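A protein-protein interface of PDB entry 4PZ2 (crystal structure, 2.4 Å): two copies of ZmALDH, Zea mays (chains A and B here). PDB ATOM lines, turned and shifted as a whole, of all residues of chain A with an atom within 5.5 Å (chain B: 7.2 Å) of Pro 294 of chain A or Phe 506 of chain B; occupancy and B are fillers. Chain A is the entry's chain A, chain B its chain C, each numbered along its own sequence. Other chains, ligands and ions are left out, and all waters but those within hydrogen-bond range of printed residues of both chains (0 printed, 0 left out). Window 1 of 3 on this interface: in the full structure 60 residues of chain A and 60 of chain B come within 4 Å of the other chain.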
ATOM      1  N   LEU A 189      -0.517  -7.699  -1.501  1.00  0.00           N
ATOM      2  CA  LEU A 189      -0.130  -6.370  -1.998  1.00  0.00           C
ATOM      3  C   LEU A 189      -1.089  -5.747  -3.034  1.00  0.00           C
ATOM      4  O   LEU A 189      -1.473  -4.585  -2.887  1.00  0.00           O
ATOM      5  CB  LEU A 189       1.324  -6.361  -2.486  1.00  0.00           C
ATOM      6  CG  LEU A 189       1.925  -5.014  -2.898  1.00  0.00           C
ATOM      7  CD1 LEU A 189       1.882  -3.982  -1.751  1.00  0.00           C
ATOM      8  CD2 LEU A 189       3.325  -5.200  -3.377  1.00  0.00           C
ATOM      9  N   ASP A 269       1.601  -2.763  -8.646  1.00  0.00           N
ATOM     10  CA  ASP A 269       2.100  -2.548  -7.291  1.00  0.00           C
ATOM     11  C   ASP A 269       3.550  -2.948  -7.047  1.00  0.00           C
ATOM     12  O   ASP A 269       4.203  -2.355  -6.180  1.00  0.00           O
ATOM     13  CB  ASP A 269       1.117  -3.106  -6.243  1.00  0.00           C
ATOM     14  CG  ASP A 269      -0.259  -2.474  -6.362  1.00  0.00           C
ATOM     15  OD1 ASP A 269      -0.348  -1.226  -6.318  1.00  0.00           O
ATOM     16  OD2 ASP A 269      -1.230  -3.214  -6.583  1.00  0.00           O
ATOM     17  N   MET A 270       4.064  -3.903  -7.856  1.00  0.00           N
ATOM     18  CA  MET A 270       5.449  -4.367  -7.809  1.00  0.00           C
ATOM     19  C   MET A 270       5.873  -5.032  -9.114  1.00  0.00           C
ATOM     20  O   MET A 270       5.033  -5.476  -9.907  1.00  0.00           O
ATOM     21  CB  MET A 270       5.725  -5.296  -6.591  1.00  0.00           C
ATOM     22  CG  MET A 270       4.902  -6.599  -6.561  1.00  0.00           C
ATOM     23  SD  MET A 270       5.495  -7.912  -7.675  1.00  0.00           S
ATOM     24  CE  MET A 270       6.990  -8.427  -6.827  1.00  0.00           C
ATOM     25  N   VAL A 271       7.196  -5.156  -9.296  1.00  0.00           N
ATOM     26  CA  VAL A 271       7.748  -5.886 -10.423  1.00  0.00           C
ATOM     27  C   VAL A 271       8.829  -6.886  -9.982  1.00  0.00           C
ATOM     28  O   VAL A 271       9.751  -6.535  -9.246  1.00  0.00           O
ATOM     29  CB  VAL A 271       8.064  -5.034 -11.712  1.00  0.00           C
ATOM     30  CG1 VAL A 271       8.931  -3.827 -11.394  1.00  0.00           C
ATOM     31  CG2 VAL A 271       8.682  -5.869 -12.846  1.00  0.00           C
ATOM     32  N   SER A 287      10.326   2.023 -13.131  1.00  0.00           N
ATOM     33  CA  SER A 287       9.662   2.229 -11.842  1.00  0.00           C
ATOM     34  C   SER A 287       9.866   3.681 -11.389  1.00  0.00           C
ATOM     35  O   SER A 287       8.899   4.345 -11.005  1.00  0.00           O
ATOM     36  CB  SER A 287      10.222   1.261 -10.807  1.00  0.00           C
ATOM     37  OG  SER A 287       9.764   1.500  -9.489  1.00  0.00           O
ATOM     38  N   LEU A 292       7.116   4.364  -8.803  1.00  0.00           N
ATOM     39  CA  LEU A 292       8.133   3.944  -7.825  1.00  0.00           C
ATOM     40  C   LEU A 292       7.760   2.645  -7.120  1.00  0.00           C
ATOM     41  O   LEU A 292       7.991   2.505  -5.919  1.00  0.00           O
ATOM     42  CB  LEU A 292       8.474   5.054  -6.797  1.00  0.00           C
ATOM     43  CG  LEU A 292       9.297   6.221  -7.307  1.00  0.00           C
ATOM     44  CD1 LEU A 292       9.023   7.433  -6.504  1.00  0.00           C
ATOM     45  CD2 LEU A 292      10.765   5.913  -7.245  1.00  0.00           C
ATOM     46  N   LYS A 293       7.167   1.704  -7.863  1.00  0.00           N
ATOM     47  CA  LYS A 293       6.789   0.373  -7.380  1.00  0.00           C
ATOM     48  C   LYS A 293       8.066  -0.383  -6.946  1.00  0.00           C
ATOM     49  O   LYS A 293       9.090  -0.244  -7.617  1.00  0.00           O
ATOM     50  CB  LYS A 293       6.059  -0.439  -8.493  1.00  0.00           C
ATOM     51  CG  LYS A 293       6.878  -0.616  -9.800  1.00  0.00           C
ATOM     52  CD  LYS A 293       6.234  -1.479 -10.898  1.00  0.00           C
ATOM     53  CE  LYS A 293       5.117  -0.867 -11.723  1.00  0.00           C
ATOM     54  NZ  LYS A 293       5.442   0.463 -12.317  1.00  0.00           N
ATOM     55  N   PRO A 294       8.059  -1.188  -5.859  1.00  0.00           N
ATOM     56  CA  PRO A 294       9.267  -1.968  -5.544  1.00  0.00           C
ATOM     57  C   PRO A 294       9.607  -2.926  -6.698  1.00  0.00           C
ATOM     58  O   PRO A 294       8.721  -3.508  -7.340  1.00  0.00           O
ATOM     59  CB  PRO A 294       8.902  -2.702  -4.247  1.00  0.00           C
ATOM     60  CG  PRO A 294       7.412  -2.644  -4.143  1.00  0.00           C
ATOM     61  CD  PRO A 294       6.953  -1.457  -4.909  1.00  0.00           C
ATOM     62  N   VAL A 295      10.905  -3.037  -6.984  1.00  0.00           N
ATOM     63  CA  VAL A 295      11.493  -3.851  -8.045  1.00  0.00           C
ATOM     64  C   VAL A 295      12.340  -4.961  -7.386  1.00  0.00           C
ATOM     65  O   VAL A 295      13.026  -4.707  -6.386  1.00  0.00           O
ATOM     66  CB  VAL A 295      12.318  -2.927  -8.988  1.00  0.00           C
ATOM     67  CG1 VAL A 295      13.144  -3.717  -9.984  1.00  0.00           C
ATOM     68  CG2 VAL A 295      11.412  -1.947  -9.728  1.00  0.00           C
ATOM     69  N   TYR A 296      12.247  -6.195  -7.926  1.00  0.00           N
ATOM     70  CA  TYR A 296      12.998  -7.361  -7.433  1.00  0.00           C
ATOM     71  C   TYR A 296      13.723  -7.935  -8.640  1.00  0.00           C
ATOM     72  O   TYR A 296      13.092  -8.201  -9.670  1.00  0.00           O
ATOM     73  CB  TYR A 296      12.065  -8.371  -6.721  1.00  0.00           C
ATOM     74  CG  TYR A 296      11.328  -7.727  -5.566  1.00  0.00           C
ATOM     75  CD1 TYR A 296      11.879  -7.707  -4.286  1.00  0.00           C
ATOM     76  CD2 TYR A 296      10.123  -7.050  -5.769  1.00  0.00           C
ATOM     77  CE1 TYR A 296      11.247  -7.039  -3.234  1.00  0.00           C
ATOM     78  CE2 TYR A 296       9.499  -6.357  -4.736  1.00  0.00           C
ATOM     79  CZ  TYR A 296      10.055  -6.368  -3.463  1.00  0.00           C
ATOM     80  OH  TYR A 296       9.406  -5.742  -2.424  1.00  0.00           O
ATOM     81  N   PHE B 273      17.064   5.380   1.651  1.00  0.00           N
ATOM     82  CA  PHE B 273      16.705   6.774   1.437  1.00  0.00           C
ATOM     83  C   PHE B 273      15.415   7.179   2.124  1.00  0.00           C
ATOM     84  O   PHE B 273      14.407   6.477   2.033  1.00  0.00           O
ATOM     85  CB  PHE B 273      16.636   7.080  -0.075  1.00  0.00           C
ATOM     86  CG  PHE B 273      16.091   8.445  -0.426  1.00  0.00           C
ATOM     87  CD1 PHE B 273      16.904   9.573  -0.362  1.00  0.00           C
ATOM     88  CD2 PHE B 273      14.759   8.608  -0.803  1.00  0.00           C
ATOM     89  CE1 PHE B 273      16.402  10.833  -0.682  1.00  0.00           C
ATOM     90  CE2 PHE B 273      14.259   9.872  -1.110  1.00  0.00           C
ATOM     91  CZ  PHE B 273      15.081  10.973  -1.045  1.00  0.00           C
ATOM     92  N   GLY B 280      13.181  10.327  -4.620  1.00  0.00           N
ATOM     93  CA  GLY B 280      13.168   8.863  -4.633  1.00  0.00           C
ATOM     94  C   GLY B 280      13.367   8.288  -6.036  1.00  0.00           C
ATOM     95  O   GLY B 280      14.060   7.280  -6.199  1.00  0.00           O
ATOM     96  N   MET B 284      16.584   5.735  -7.365  1.00  0.00           N
ATOM     97  CA  MET B 284      16.335   4.541  -8.165  1.00  0.00           C
ATOM     98  C   MET B 284      17.088   4.594  -9.477  1.00  0.00           C
ATOM     99  O   MET B 284      17.610   3.567  -9.910  1.00  0.00           O
ATOM    100  CB  MET B 284      14.842   4.357  -8.422  1.00  0.00           C
ATOM    101  CG  MET B 284      14.135   3.664  -7.289  1.00  0.00           C
ATOM    102  SD  MET B 284      12.646   2.812  -7.854  1.00  0.00           S
ATOM    103  CE  MET B 284      13.320   1.357  -8.593  1.00  0.00           C
ATOM    104  N   PRO B 294      20.473  -2.592  -4.139  1.00  0.00           N
ATOM    105  CA  PRO B 294      19.083  -2.468  -3.668  1.00  0.00           C
ATOM    106  C   PRO B 294      18.851  -1.087  -3.028  1.00  0.00           C
ATOM    107  O   PRO B 294      19.719  -0.535  -2.344  1.00  0.00           O
ATOM    108  CB  PRO B 294      18.921  -3.626  -2.673  1.00  0.00           C
ATOM    109  CG  PRO B 294      20.316  -4.060  -2.322  1.00  0.00           C
ATOM    110  CD  PRO B 294      21.190  -3.704  -3.475  1.00  0.00           C
ATOM    111  N   VAL B 295      17.693  -0.517  -3.323  1.00  0.00           N
ATOM    112  CA  VAL B 295      17.236   0.792  -2.876  1.00  0.00           C
ATOM    113  C   VAL B 295      16.010   0.596  -1.962  1.00  0.00           C
ATOM    114  O   VAL B 295      15.162  -0.265  -2.224  1.00  0.00           O
ATOM    115  CB  VAL B 295      16.935   1.676  -4.124  1.00  0.00           C
ATOM    116  CG1 VAL B 295      16.246   2.974  -3.754  1.00  0.00           C
ATOM    117  CG2 VAL B 295      18.208   1.976  -4.896  1.00  0.00           C
ATOM    118  N   TYR B 296      15.959   1.350  -0.854  1.00  0.00           N
ATOM    119  CA  TYR B 296      14.873   1.296   0.135  1.00  0.00           C
ATOM    120  C   TYR B 296      14.404   2.717   0.310  1.00  0.00           C
ATOM    121  O   TYR B 296      15.215   3.603   0.614  1.00  0.00           O
ATOM    122  CB  TYR B 296      15.334   0.632   1.452  1.00  0.00           C
ATOM    123  CG  TYR B 296      15.861  -0.767   1.220  1.00  0.00           C
ATOM    124  CD1 TYR B 296      15.009  -1.868   1.246  1.00  0.00           C
ATOM    125  CD2 TYR B 296      17.200  -0.983   0.895  1.00  0.00           C
ATOM    126  CE1 TYR B 296      15.476  -3.149   0.953  1.00  0.00           C
ATOM    127  CE2 TYR B 296      17.670  -2.251   0.574  1.00  0.00           C
ATOM    128  CZ  TYR B 296      16.809  -3.335   0.616  1.00  0.00           C
ATOM    129  OH  TYR B 296      17.303  -4.599   0.373  1.00  0.00           O
ATOM    130  N   LEU B 297      13.119   2.958   0.005  1.00  0.00           N
ATOM    131  CA  LEU B 297      12.545   4.309  -0.031  1.00  0.00           C
ATOM    132  C   LEU B 297      11.454   4.590   0.991  1.00  0.00           C
ATOM    133  O   LEU B 297      10.444   3.898   1.021  1.00  0.00           O
ATOM    134  CB  LEU B 297      12.034   4.624  -1.463  1.00  0.00           C
ATOM    135  CG  LEU B 297      13.023   4.473  -2.624  1.00  0.00           C
ATOM    136  CD1 LEU B 297      12.309   4.647  -3.962  1.00  0.00           C
ATOM    137  CD2 LEU B 297      14.164   5.474  -2.506  1.00  0.00           C
ATOM    138  N   GLU B 298      11.657   5.644   1.799  1.00  0.00           N
ATOM    139  CA  GLU B 298      10.758   6.143   2.850  1.00  0.00           C
ATOM    140  C   GLU B 298      10.362   7.504   2.361  1.00  0.00           C
ATOM    141  O   GLU B 298      11.114   8.471   2.501  1.00  0.00           O
ATOM    142  CB  GLU B 298      11.513   6.248   4.185  1.00  0.00           C
ATOM    143  CG  GLU B 298      11.832   4.915   4.836  1.00  0.00           C
ATOM    144  CD  GLU B 298      10.686   4.237   5.571  1.00  0.00           C
ATOM    145  OE1 GLU B 298      10.834   3.036   5.882  1.00  0.00           O
ATOM    146  OE2 GLU B 298       9.648   4.887   5.838  1.00  0.00           O
ATOM    147  N   LEU B 299       9.224   7.566   1.678  1.00  0.00           N
ATOM    148  CA  LEU B 299       8.812   8.777   0.984  1.00  0.00           C
ATOM    149  C   LEU B 299       7.742   9.648   1.659  1.00  0.00           C
ATOM    150  O   LEU B 299       7.508   9.508   2.858  1.00  0.00           O
ATOM    151  CB  LEU B 299       8.560   8.444  -0.497  1.00  0.00           C
ATOM    152  CG  LEU B 299       9.632   7.558  -1.173  1.00  0.00           C
ATOM    153  CD1 LEU B 299       9.213   7.129  -2.569  1.00  0.00           C
ATOM    154  CD2 LEU B 299      11.013   8.218  -1.168  1.00  0.00           C
ATOM    155  N   PHE B 498       8.126   0.622  10.366  1.00  0.00           N
ATOM    156  CA  PHE B 498       7.624   1.822   9.710  1.00  0.00           C
ATOM    157  C   PHE B 498       8.069   1.879   8.246  1.00  0.00           C
ATOM    158  O   PHE B 498       9.269   1.918   7.947  1.00  0.00           O
ATOM    159  CB  PHE B 498       8.063   3.089  10.464  1.00  0.00           C
ATOM    160  CG  PHE B 498       7.483   4.372   9.899  1.00  0.00           C
ATOM    161  CD1 PHE B 498       6.223   4.819  10.290  1.00  0.00           C
ATOM    162  CD2 PHE B 498       8.197   5.134   8.976  1.00  0.00           C
ATOM    163  CE1 PHE B 498       5.685   5.997   9.760  1.00  0.00           C
ATOM    164  CE2 PHE B 498       7.658   6.308   8.448  1.00  0.00           C
ATOM    165  CZ  PHE B 498       6.416   6.742   8.856  1.00  0.00           C
ATOM    166  N   GLY B 499       7.094   1.951   7.359  1.00  0.00           N
ATOM    167  CA  GLY B 499       7.335   2.018   5.933  1.00  0.00           C
ATOM    168  C   GLY B 499       6.093   2.321   5.136  1.00  0.00           C
ATOM    169  O   GLY B 499       4.974   2.063   5.591  1.00  0.00           O
ATOM    170  N   GLY B 500       6.295   2.867   3.941  1.00  0.00           N
ATOM    171  CA  GLY B 500       5.192   3.244   3.080  1.00  0.00           C
ATOM    172  C   GLY B 500       4.614   2.128   2.249  1.00  0.00           C
ATOM    173  O   GLY B 500       5.122   1.005   2.226  1.00  0.00           O
ATOM    174  N   ARG B 501       3.512   2.464   1.573  1.00  0.00           N
ATOM    175  CA  ARG B 501       2.788   1.668   0.590  1.00  0.00           C
ATOM    176  C   ARG B 501       2.534   2.647  -0.557  1.00  0.00           C
ATOM    177  O   ARG B 501       2.576   3.869  -0.344  1.00  0.00           O
ATOM    178  CB  ARG B 501       1.480   1.133   1.182  1.00  0.00           C
ATOM    179  CG  ARG B 501       0.918  -0.021   0.408  1.00  0.00           C
ATOM    180  CD  ARG B 501      -0.194  -0.718   1.135  1.00  0.00           C
ATOM    181  NE  ARG B 501      -0.879  -1.654   0.243  1.00  0.00           N
ATOM    182  CZ  ARG B 501      -1.836  -2.491   0.613  1.00  0.00           C
ATOM    183  NH1 ARG B 501      -2.239  -2.532   1.876  1.00  0.00           N
ATOM    184  NH2 ARG B 501      -2.400  -3.296  -0.278  1.00  0.00           N
ATOM    185  N   LYS B 502       2.307   2.131  -1.768  1.00  0.00           N
ATOM    186  CA  LYS B 502       2.070   2.953  -2.965  1.00  0.00           C
ATOM    187  C   LYS B 502       3.241   3.950  -3.192  1.00  0.00           C
ATOM    188  O   LYS B 502       4.394   3.515  -3.091  1.00  0.00           O
ATOM    189  CB  LYS B 502       0.690   3.617  -2.915  1.00  0.00           C
ATOM    190  CG  LYS B 502      -0.477   2.638  -2.869  1.00  0.00           C
ATOM    191  CD  LYS B 502      -1.701   3.238  -2.127  1.00  0.00           C
ATOM    192  CE  LYS B 502      -2.353   4.381  -2.875  1.00  0.00           C
ATOM    193  NZ  LYS B 502      -3.661   4.769  -2.280  1.00  0.00           N
ATOM    194  N   MET B 503       2.984   5.258  -3.445  1.00  0.00           N
ATOM    195  CA  MET B 503       4.073   6.230  -3.661  1.00  0.00           C
ATOM    196  C   MET B 503       4.742   6.794  -2.399  1.00  0.00           C
ATOM    197  O   MET B 503       5.568   7.706  -2.488  1.00  0.00           O
ATOM    198  CB  MET B 503       3.717   7.294  -4.684  1.00  0.00           C
ATOM    199  CG  MET B 503       3.433   6.703  -6.047  1.00  0.00           C
ATOM    200  SD  MET B 503       3.513   7.872  -7.389  1.00  0.00           S
ATOM    201  CE  MET B 503       2.098   7.421  -8.157  1.00  0.00           C
ATOM    202  N   SER B 504       4.445   6.202  -1.238  1.00  0.00           N
ATOM    203  CA  SER B 504       5.075   6.567   0.025  1.00  0.00           C
ATOM    204  C   SER B 504       6.316   5.679   0.258  1.00  0.00           C
ATOM    205  O   SER B 504       7.039   5.856   1.247  1.00  0.00           O
ATOM    206  CB  SER B 504       4.085   6.470   1.175  1.00  0.00           C
ATOM    207  OG  SER B 504       3.189   7.568   1.099  1.00  0.00           O
ATOM    208  N   GLY B 505       6.537   4.745  -0.672  1.00  0.00           N
ATOM    209  CA  GLY B 505       7.708   3.884  -0.686  1.00  0.00           C
ATOM    210  C   GLY B 505       7.526   2.418  -0.385  1.00  0.00           C
ATOM    211  O   GLY B 505       6.425   1.859  -0.497  1.00  0.00           O
ATOM    212  N   PHE B 506       8.646   1.802  -0.002  1.00  0.00           N
ATOM    213  CA  PHE B 506       8.803   0.387   0.325  1.00  0.00           C
ATOM    214  C   PHE B 506      10.049   0.229   1.219  1.00  0.00           C
ATOM    215  O   PHE B 506      11.002   1.014   1.106  1.00  0.00           O
ATOM    216  CB  PHE B 506       8.948  -0.450  -0.966  1.00  0.00           C
ATOM    217  CG  PHE B 506       9.883   0.134  -2.022  1.00  0.00           C
ATOM    218  CD1 PHE B 506      11.262  -0.062  -1.947  1.00  0.00           C
ATOM    219  CD2 PHE B 506       9.381   0.861  -3.094  1.00  0.00           C
ATOM    220  CE1 PHE B 506      12.113   0.477  -2.912  1.00  0.00           C
ATOM    221  CE2 PHE B 506      10.239   1.397  -4.059  1.00  0.00           C
ATOM    222  CZ  PHE B 506      11.593   1.188  -3.971  1.00  0.00           C
ATOM    223  N   GLY B 507      10.029  -0.781   2.088  1.00  0.00           N
ATOM    224  CA  GLY B 507      11.115  -1.049   3.018  1.00  0.00           C
ATOM    225  C   GLY B 507      10.747  -0.572   4.409  1.00  0.00           C
ATOM    226  O   GLY B 507      10.015   0.410   4.558  1.00  0.00           O
ATOM    227  N   LYS B 508      11.241  -1.266   5.436  1.00  0.00           N
ATOM    228  CA  LYS B 508      10.912  -0.911   6.812  1.00  0.00           C
ATOM    229  C   LYS B 508      12.054  -0.306   7.600  1.00  0.00           C
ATOM    230  O   LYS B 508      13.177  -0.795   7.524  1.00  0.00           O
ATOM    231  CB  LYS B 508      10.363  -2.136   7.575  1.00  0.00           C
ATOM    232  CG  LYS B 508       9.098  -2.747   6.993  1.00  0.00           C
ATOM    233  CD  LYS B 508       7.879  -1.846   7.087  1.00  0.00           C
ATOM    234  CE  LYS B 508       6.673  -2.505   6.448  1.00  0.00           C
ATOM    235  NZ  LYS B 508       5.547  -1.546   6.199  1.00  0.00           N
ATOM    236  N   LYS B 517      17.392  -5.224   5.111  1.00  0.00           N
ATOM    237  CA  LYS B 517      18.039  -4.405   4.096  1.00  0.00           C
ATOM    238  C   LYS B 517      19.569  -4.333   4.215  1.00  0.00           C
ATOM    239  O   LYS B 517      20.234  -4.053   3.217  1.00  0.00           O
ATOM    240  CB  LYS B 517      17.392  -3.017   4.045  1.00  0.00           C
ATOM    241  CG  LYS B 517      17.843  -2.033   5.110  1.00  0.00           C
ATOM    242  CD  LYS B 517      17.218  -0.640   4.972  1.00  0.00           C
ATOM    243  CE  LYS B 517      15.808  -0.534   5.488  1.00  0.00           C
ATOM    244  NZ  LYS B 517      15.771  -0.645   6.959  1.00  0.00           N
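Of the 10 printed residues of chain A, 5 touch a printed residue of chain B.
Of the 21 printed residues of chain B, 6 touch a printed residue of chain A.
Printed residues of chain B that touch a printed residue of chain A: Gly 280, Met 284, Leu 297, Leu 299, Arg 501 and Phe 506.
Hydrophobic or aromatic side chains of chain B within 4 Å of the printed part of chain A: Met 284, Leu 297, Leu 299 and Phe 506.
Among the printed residues, 9 pairs touch across the chains.
Among the printed residues, no Asp or Glu carboxylate lies within 4 Å of a Lys or Arg side-chain nitrogen of the other chain.
N of Val 271 of chain A sits at hydrogen-bond distance from O of Pro 294 of chain A (3.0 Å).
The backbone carbonyl oxygen (O) of Leu 297 of chain B lies within hydrogen-bond range of the backbone NH (N) of Phe 506 of chain B, 2.9 Å away.
N of Leu 299 of chain B lies within hydrogen-bond range of O of Ser 504 of chain B (2.8 Å).
The side-chain hydroxyl (OG) of Ser 287 of chain A is in hydrogen-bond range of the backbone carbonyl oxygen (O) of Lys 293 of chain A (2.6 Å).
O of Ser 287 of chain A sits at hydrogen-bond distance from N of Leu 292 of chain A.
NH2 of Arg 501 of chain B sits at hydrogen-bond distance from O of Leu 189 of chain A (3.1 Å).
The side-chain hydroxyl of Ser 287 of chain A is in hydrogen-bond range of the side-chain sulfur of Met 284 of chain B.
Gly 280 of chain B touches Leu 292 of chain A.
Met 284 of chain B touches Leu 292 of chain A.
Leu 292 of chain A touches Leu 297 of chain B (CD2 to CD1, 3.8 Å).
CD1 of Leu 292 of chain A touches CD1 of Leu 299 of chain B, 3.95 Å away.
O of Leu 292 of chain A touches CE2 of Phe 506 of chain B (3.1 Å).
N of Pro 294 of chain A touches CD2 of Phe 506 of chain B, at 3.7 Å.
Val 295 of chain A touches Met 284 of chain B (CG2 to CE, 3.98 Å).
Of the printed residues of chain B, Leu 189 of chain A touches Arg 501.
Of the printed residues of chain B, Leu 292 of chain A touches Gly 280, Met 284, Leu 297, Leu 299 and Phe 506.
Of chain B, only Phe 506 (3.7 Å) comes within 4 Å of Pro 294 of chain A.
Printed residues of chain A within 4 Å of Gly 280 of chain B: Leu 292.
Of the printed residues of chain A, Met 284 of chain B touches Ser 287, Leu 292 and Val 295.
Phe 506 of chain B touches just these residues of chain A: Leu 292 and Pro 294.
The nearest residue of chain B that does not touch Pro 294 of chain A is Gly 505 of chain B (5.5 Å).
Positions printed for both chains: 294, 295 and 296.
Of the 9 pairs that touch across the chains among the printed residues, none has its exchanged pair printed and touching as well.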
